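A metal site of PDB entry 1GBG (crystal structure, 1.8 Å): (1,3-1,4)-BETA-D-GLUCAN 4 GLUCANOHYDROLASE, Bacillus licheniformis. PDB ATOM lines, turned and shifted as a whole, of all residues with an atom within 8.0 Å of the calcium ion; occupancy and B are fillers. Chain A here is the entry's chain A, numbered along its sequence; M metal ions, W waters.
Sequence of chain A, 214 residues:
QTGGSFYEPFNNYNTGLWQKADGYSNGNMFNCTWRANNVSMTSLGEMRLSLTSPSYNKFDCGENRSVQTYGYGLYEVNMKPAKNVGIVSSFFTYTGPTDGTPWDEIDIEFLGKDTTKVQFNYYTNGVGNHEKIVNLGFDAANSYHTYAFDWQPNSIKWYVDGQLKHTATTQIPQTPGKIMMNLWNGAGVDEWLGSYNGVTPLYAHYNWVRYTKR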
ATOM      1  N   TYR A   7     -22.005   9.274  10.348  1.00  0.00           N
ATOM      2  CA  TYR A   7     -20.561   9.218  10.360  1.00  0.00           C
ATOM      3  C   TYR A   7     -20.096  10.401  11.198  1.00  0.00           C
ATOM      4  O   TYR A   7     -20.448  11.551  10.896  1.00  0.00           O
ATOM      5  CB  TYR A   7     -19.916   9.218   8.961  1.00  0.00           C
ATOM      6  CG  TYR A   7     -18.422   9.442   9.035  1.00  0.00           C
ATOM      7  CD1 TYR A   7     -17.602   8.445   9.568  1.00  0.00           C
ATOM      8  CD2 TYR A   7     -17.827  10.611   8.561  1.00  0.00           C
ATOM      9  CE1 TYR A   7     -16.230   8.623   9.666  1.00  0.00           C
ATOM     10  CE2 TYR A   7     -16.450  10.796   8.628  1.00  0.00           C
ATOM     11  CZ  TYR A   7     -15.643   9.784   9.148  1.00  0.00           C
ATOM     12  OH  TYR A   7     -14.282   9.987   9.221  1.00  0.00           O
ATOM     13  N   GLU A   8     -19.312  10.132  12.239  1.00  0.00           N
ATOM     14  CA  GLU A   8     -18.809  11.166  13.130  1.00  0.00           C
ATOM     15  C   GLU A   8     -17.294  11.279  13.053  1.00  0.00           C
ATOM     16  O   GLU A   8     -16.564  10.435  13.570  1.00  0.00           O
ATOM     17  CB  GLU A   8     -19.295  10.896  14.561  1.00  0.00           C
ATOM     18  CG  GLU A   8     -18.689  11.824  15.633  1.00  0.00           C
ATOM     19  CD  GLU A   8     -19.013  13.266  15.376  1.00  0.00           C
ATOM     20  OE1 GLU A   8     -20.182  13.630  15.833  1.00  0.00           O
ATOM     21  OE2 GLU A   8     -18.274  13.991  14.748  1.00  0.00           O
ATOM     22  N   PRO A   9     -16.815  12.332  12.393  1.00  0.00           N
ATOM     23  CA  PRO A   9     -15.397  12.549  12.251  1.00  0.00           C
ATOM     24  C   PRO A   9     -14.761  13.329  13.404  1.00  0.00           C
ATOM     25  O   PRO A   9     -13.540  13.441  13.501  1.00  0.00           O
ATOM     26  CB  PRO A   9     -15.250  13.338  10.948  1.00  0.00           C
ATOM     27  CG  PRO A   9     -16.591  14.030  10.722  1.00  0.00           C
ATOM     28  CD  PRO A   9     -17.606  13.297  11.591  1.00  0.00           C
ATOM     29  N   PHE A  10     -15.589  13.875  14.285  1.00  0.00           N
ATOM     30  CA  PHE A  10     -15.101  14.630  15.424  1.00  0.00           C
ATOM     31  C   PHE A  10     -14.328  15.876  15.050  1.00  0.00           C
ATOM     32  O   PHE A  10     -13.226  16.113  15.561  1.00  0.00           O
ATOM     33  CB  PHE A  10     -14.295  13.758  16.418  1.00  0.00           C
ATOM     34  CG  PHE A  10     -15.194  12.892  17.256  1.00  0.00           C
ATOM     35  CD1 PHE A  10     -16.325  13.421  17.864  1.00  0.00           C
ATOM     36  CD2 PHE A  10     -14.912  11.530  17.422  1.00  0.00           C
ATOM     37  CE1 PHE A  10     -17.168  12.633  18.647  1.00  0.00           C
ATOM     38  CE2 PHE A  10     -15.746  10.712  18.200  1.00  0.00           C
ATOM     39  CZ  PHE A  10     -16.863  11.274  18.798  1.00  0.00           C
ATOM     40  N   ASN A  11     -14.910  16.681  14.170  1.00  0.00           N
ATOM     41  CA  ASN A  11     -14.312  17.929  13.731  1.00  0.00           C
ATOM     42  C   ASN A  11     -14.751  19.048  14.653  1.00  0.00           C
ATOM     43  O   ASN A  11     -14.199  20.144  14.671  1.00  0.00           O
ATOM     44  CB  ASN A  11     -14.731  18.265  12.280  1.00  0.00           C
ATOM     45  CG  ASN A  11     -13.934  17.458  11.289  1.00  0.00           C
ATOM     46  OD1 ASN A  11     -12.774  17.101  11.544  1.00  0.00           O
ATOM     47  ND2 ASN A  11     -14.571  17.127  10.170  1.00  0.00           N
ATOM     48  N   ASN A  12     -15.785  18.720  15.411  1.00  0.00           N
ATOM     49  CA  ASN A  12     -16.404  19.596  16.379  1.00  0.00           C
ATOM     50  C   ASN A  12     -17.226  18.744  17.328  1.00  0.00           C
ATOM     51  O   ASN A  12     -17.322  17.540  17.115  1.00  0.00           O
ATOM     52  CB  ASN A  12     -17.280  20.671  15.681  1.00  0.00           C
ATOM     53  CG  ASN A  12     -18.610  20.168  15.134  1.00  0.00           C
ATOM     54  OD1 ASN A  12     -18.695  19.200  14.376  1.00  0.00           O
ATOM     55  ND2 ASN A  12     -19.694  20.868  15.481  1.00  0.00           N
ATOM     56  N   MET A  41     -12.602  18.263  22.924  1.00  0.00           N
ATOM     57  CA  MET A  41     -12.108  18.078  21.565  1.00  0.00           C
ATOM     58  C   MET A  41     -10.666  18.519  21.431  1.00  0.00           C
ATOM     59  O   MET A  41     -10.266  19.517  22.029  1.00  0.00           O
ATOM     60  CB  MET A  41     -12.943  18.901  20.567  1.00  0.00           C
ATOM     61  CG  MET A  41     -14.441  18.684  20.688  1.00  0.00           C
ATOM     62  SD  MET A  41     -14.894  16.950  20.470  1.00  0.00           S
ATOM     63  CE  MET A  41     -14.265  16.608  18.806  1.00  0.00           C
ATOM     64  N   THR A  42      -9.885  17.789  20.646  1.00  0.00           N
ATOM     65  CA  THR A  42      -8.488  18.146  20.435  1.00  0.00           C
ATOM     66  C   THR A  42      -8.353  18.934  19.140  1.00  0.00           C
ATOM     67  O   THR A  42      -9.236  18.937  18.282  1.00  0.00           O
ATOM     68  CB  THR A  42      -7.568  16.932  20.380  1.00  0.00           C
ATOM     69  OG1 THR A  42      -7.807  16.216  19.178  1.00  0.00           O
ATOM     70  CG2 THR A  42      -7.767  16.046  21.605  1.00  0.00           C
ATOM     71  N   LEU A  44      -6.447  18.226  16.829  1.00  0.00           N
ATOM     72  CA  LEU A  44      -6.250  17.250  15.781  1.00  0.00           C
ATOM     73  C   LEU A  44      -7.528  16.555  15.326  1.00  0.00           C
ATOM     74  O   LEU A  44      -7.477  15.570  14.594  1.00  0.00           O
ATOM     75  CB  LEU A  44      -5.187  16.188  16.123  1.00  0.00           C
ATOM     76  CG  LEU A  44      -3.766  16.744  16.170  1.00  0.00           C
ATOM     77  CD1 LEU A  44      -2.848  15.699  16.794  1.00  0.00           C
ATOM     78  CD2 LEU A  44      -3.285  17.056  14.755  1.00  0.00           C
ATOM     79  N   GLY A  45      -8.693  17.059  15.741  1.00  0.00           N
ATOM     80  CA  GLY A  45      -9.943  16.451  15.338  1.00  0.00           C
ATOM     81  C   GLY A  45     -10.248  15.120  16.025  1.00  0.00           C
ATOM     82  O   GLY A  45     -10.625  14.134  15.400  1.00  0.00           O
ATOM     83  N   GLU A  46     -10.098  15.108  17.349  1.00  0.00           N
ATOM     84  CA  GLU A  46     -10.386  13.895  18.102  1.00  0.00           C
ATOM     85  C   GLU A  46     -11.179  14.231  19.342  1.00  0.00           C
ATOM     86  O   GLU A  46     -11.097  15.341  19.859  1.00  0.00           O
ATOM     87  CB  GLU A  46      -9.133  13.133  18.560  1.00  0.00           C
ATOM     88  CG  GLU A  46      -8.025  13.009  17.498  1.00  0.00           C
ATOM     89  CD  GLU A  46      -6.644  13.034  18.098  1.00  0.00           C
ATOM     90  OE1 GLU A  46      -6.311  13.772  19.011  1.00  0.00           O
ATOM     91  OE2 GLU A  46      -5.836  12.193  17.506  1.00  0.00           O
ATOM     92  N   MET A  47     -11.949  13.271  19.826  1.00  0.00           N
ATOM     93  CA  MET A  47     -12.697  13.501  21.044  1.00  0.00           C
ATOM     94  C   MET A  47     -11.824  12.872  22.108  1.00  0.00           C
ATOM     95  O   MET A  47     -11.338  11.749  21.944  1.00  0.00           O
ATOM     96  CB  MET A  47     -14.097  12.869  21.081  1.00  0.00           C
ATOM     97  CG  MET A  47     -14.726  13.066  22.457  1.00  0.00           C
ATOM     98  SD  MET A  47     -16.348  12.286  22.615  1.00  0.00           S
ATOM     99  CE  MET A  47     -15.836  10.560  22.757  1.00  0.00           C
ATOM    100  N   ASN A  78     -12.895   4.125  15.872  1.00  0.00           N
ATOM    101  CA  ASN A  78     -11.460   4.206  15.632  1.00  0.00           C
ATOM    102  C   ASN A  78     -10.953   4.909  16.883  1.00  0.00           C
ATOM    103  O   ASN A  78     -11.265   6.091  17.097  1.00  0.00           O
ATOM    104  CB  ASN A  78     -11.127   4.968  14.337  1.00  0.00           C
ATOM    105  CG  ASN A  78      -9.654   4.937  13.971  1.00  0.00           C
ATOM    106  OD1 ASN A  78      -8.950   5.921  14.193  1.00  0.00           O
ATOM    107  ND2 ASN A  78      -9.184   3.825  13.409  1.00  0.00           N
ATOM    108  N   TYR A 144      -3.945   4.147  16.681  1.00  0.00           N
ATOM    109  CA  TYR A 144      -5.347   4.017  16.385  1.00  0.00           C
ATOM    110  C   TYR A 144      -5.654   2.744  15.606  1.00  0.00           C
ATOM    111  O   TYR A 144      -4.913   2.342  14.711  1.00  0.00           O
ATOM    112  CB  TYR A 144      -5.870   5.210  15.581  1.00  0.00           C
ATOM    113  CG  TYR A 144      -6.067   6.446  16.420  1.00  0.00           C
ATOM    114  CD1 TYR A 144      -7.236   6.644  17.160  1.00  0.00           C
ATOM    115  CD2 TYR A 144      -5.072   7.428  16.447  1.00  0.00           C
ATOM    116  CE1 TYR A 144      -7.414   7.800  17.918  1.00  0.00           C
ATOM    117  CE2 TYR A 144      -5.231   8.590  17.209  1.00  0.00           C
ATOM    118  CZ  TYR A 144      -6.405   8.765  17.950  1.00  0.00           C
ATOM    119  OH  TYR A 144      -6.545   9.917  18.687  1.00  0.00           O
ATOM    120  N   TYR A 206     -10.725   9.277  20.778  1.00  0.00           N
ATOM    121  CA  TYR A 206     -11.644   8.734  19.790  1.00  0.00           C
ATOM    122  C   TYR A 206     -11.487   9.550  18.508  1.00  0.00           C
ATOM    123  O   TYR A 206     -11.751  10.742  18.506  1.00  0.00           O
ATOM    124  CB  TYR A 206     -13.095   8.727  20.289  1.00  0.00           C
ATOM    125  CG  TYR A 206     -13.223   7.881  21.529  1.00  0.00           C
ATOM    126  CD1 TYR A 206     -12.718   8.340  22.749  1.00  0.00           C
ATOM    127  CD2 TYR A 206     -13.836   6.624  21.499  1.00  0.00           C
ATOM    128  CE1 TYR A 206     -12.806   7.574  23.910  1.00  0.00           C
ATOM    129  CE2 TYR A 206     -13.939   5.843  22.647  1.00  0.00           C
ATOM    130  CZ  TYR A 206     -13.424   6.314  23.858  1.00  0.00           C
ATOM    131  OH  TYR A 206     -13.509   5.565  24.987  1.00  0.00           O
ATOM    132  N   ASN A 207     -11.051   8.877  17.455  1.00  0.00           N
ATOM    133  CA  ASN A 207     -10.831   9.499  16.164  1.00  0.00           C
ATOM    134  C   ASN A 207     -12.101   9.664  15.328  1.00  0.00           C
ATOM    135  O   ASN A 207     -12.385  10.732  14.781  1.00  0.00           O
ATOM    136  CB  ASN A 207      -9.725   8.748  15.423  1.00  0.00           C
ATOM    137  CG  ASN A 207      -9.177   9.538  14.264  1.00  0.00           C
ATOM    138  OD1 ASN A 207      -9.357  10.754  14.146  1.00  0.00           O
ATOM    139  ND2 ASN A 207      -8.545   8.839  13.356  1.00  0.00           N
ATOM    140  N   TRP A 208     -12.888   8.597  15.237  1.00  0.00           N
ATOM    141  CA  TRP A 208     -14.115   8.648  14.483  1.00  0.00           C
ATOM    142  C   TRP A 208     -15.046   7.517  14.899  1.00  0.00           C
ATOM    143  O   TRP A 208     -14.587   6.495  15.414  1.00  0.00           O
ATOM    144  CB  TRP A 208     -13.914   8.690  12.936  1.00  0.00           C
ATOM    145  CG  TRP A 208     -13.184   7.527  12.320  1.00  0.00           C
ATOM    146  CD1 TRP A 208     -11.871   7.514  11.984  1.00  0.00           C
ATOM    147  CD2 TRP A 208     -13.705   6.258  11.911  1.00  0.00           C
ATOM    148  NE1 TRP A 208     -11.534   6.308  11.417  1.00  0.00           N
ATOM    149  CE2 TRP A 208     -12.647   5.522  11.353  1.00  0.00           C
ATOM    150  CE3 TRP A 208     -14.973   5.661  11.978  1.00  0.00           C
ATOM    151  CZ2 TRP A 208     -12.813   4.221  10.872  1.00  0.00           C
ATOM    152  CZ3 TRP A 208     -15.146   4.390  11.492  1.00  0.00           C
ATOM    153  CH2 TRP A 208     -14.076   3.679  10.946  1.00  0.00           C
ATOM    154  N   VAL A 209     -16.335   7.734  14.675  1.00  0.00           N
ATOM    155  CA  VAL A 209     -17.382   6.759  14.997  1.00  0.00           C
ATOM    156  C   VAL A 209     -18.351   6.645  13.826  1.00  0.00           C
ATOM    157  O   VAL A 209     -18.667   7.625  13.155  1.00  0.00           O
ATOM    158  CB  VAL A 209     -18.137   7.120  16.275  1.00  0.00           C
ATOM    159  CG1 VAL A 209     -19.302   6.150  16.462  1.00  0.00           C
ATOM    160  CG2 VAL A 209     -17.201   7.054  17.473  1.00  0.00           C
HETATM  161 CA    CA M   1     -11.118  12.610  13.393  1.00  0.00          CA
HETATM  162  O   HOH W   1     -11.479  15.150  12.175  1.00  0.00           O
HETATM  163  O   HOH W   2      -9.018  13.840  12.491  1.00  0.00           O
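The backbone carbonyl oxygen (O) of Asn 78 sits at hydrogen-bond distance from the backbone NH (N) of Asn 207 (2.8 Å).
Three residues have an atom within 4 Å of the calcium ion: Pro 9, Gly 45 and Asn 207.
O of Pro 9 is bound to the calcium ion (2.6 Å).
O of Gly 45 is bound to the calcium ion (2.6 Å).
The calcium ion is bound by water W2 (2.6 Å).
The calcium ion is bound by the backbone carbonyl oxygen (O) of Asn 207 (2.7 Å).
OD1 of Asn 207 binds the calcium ion, 2.7 Å away.
The calcium ion is bound by water W1.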
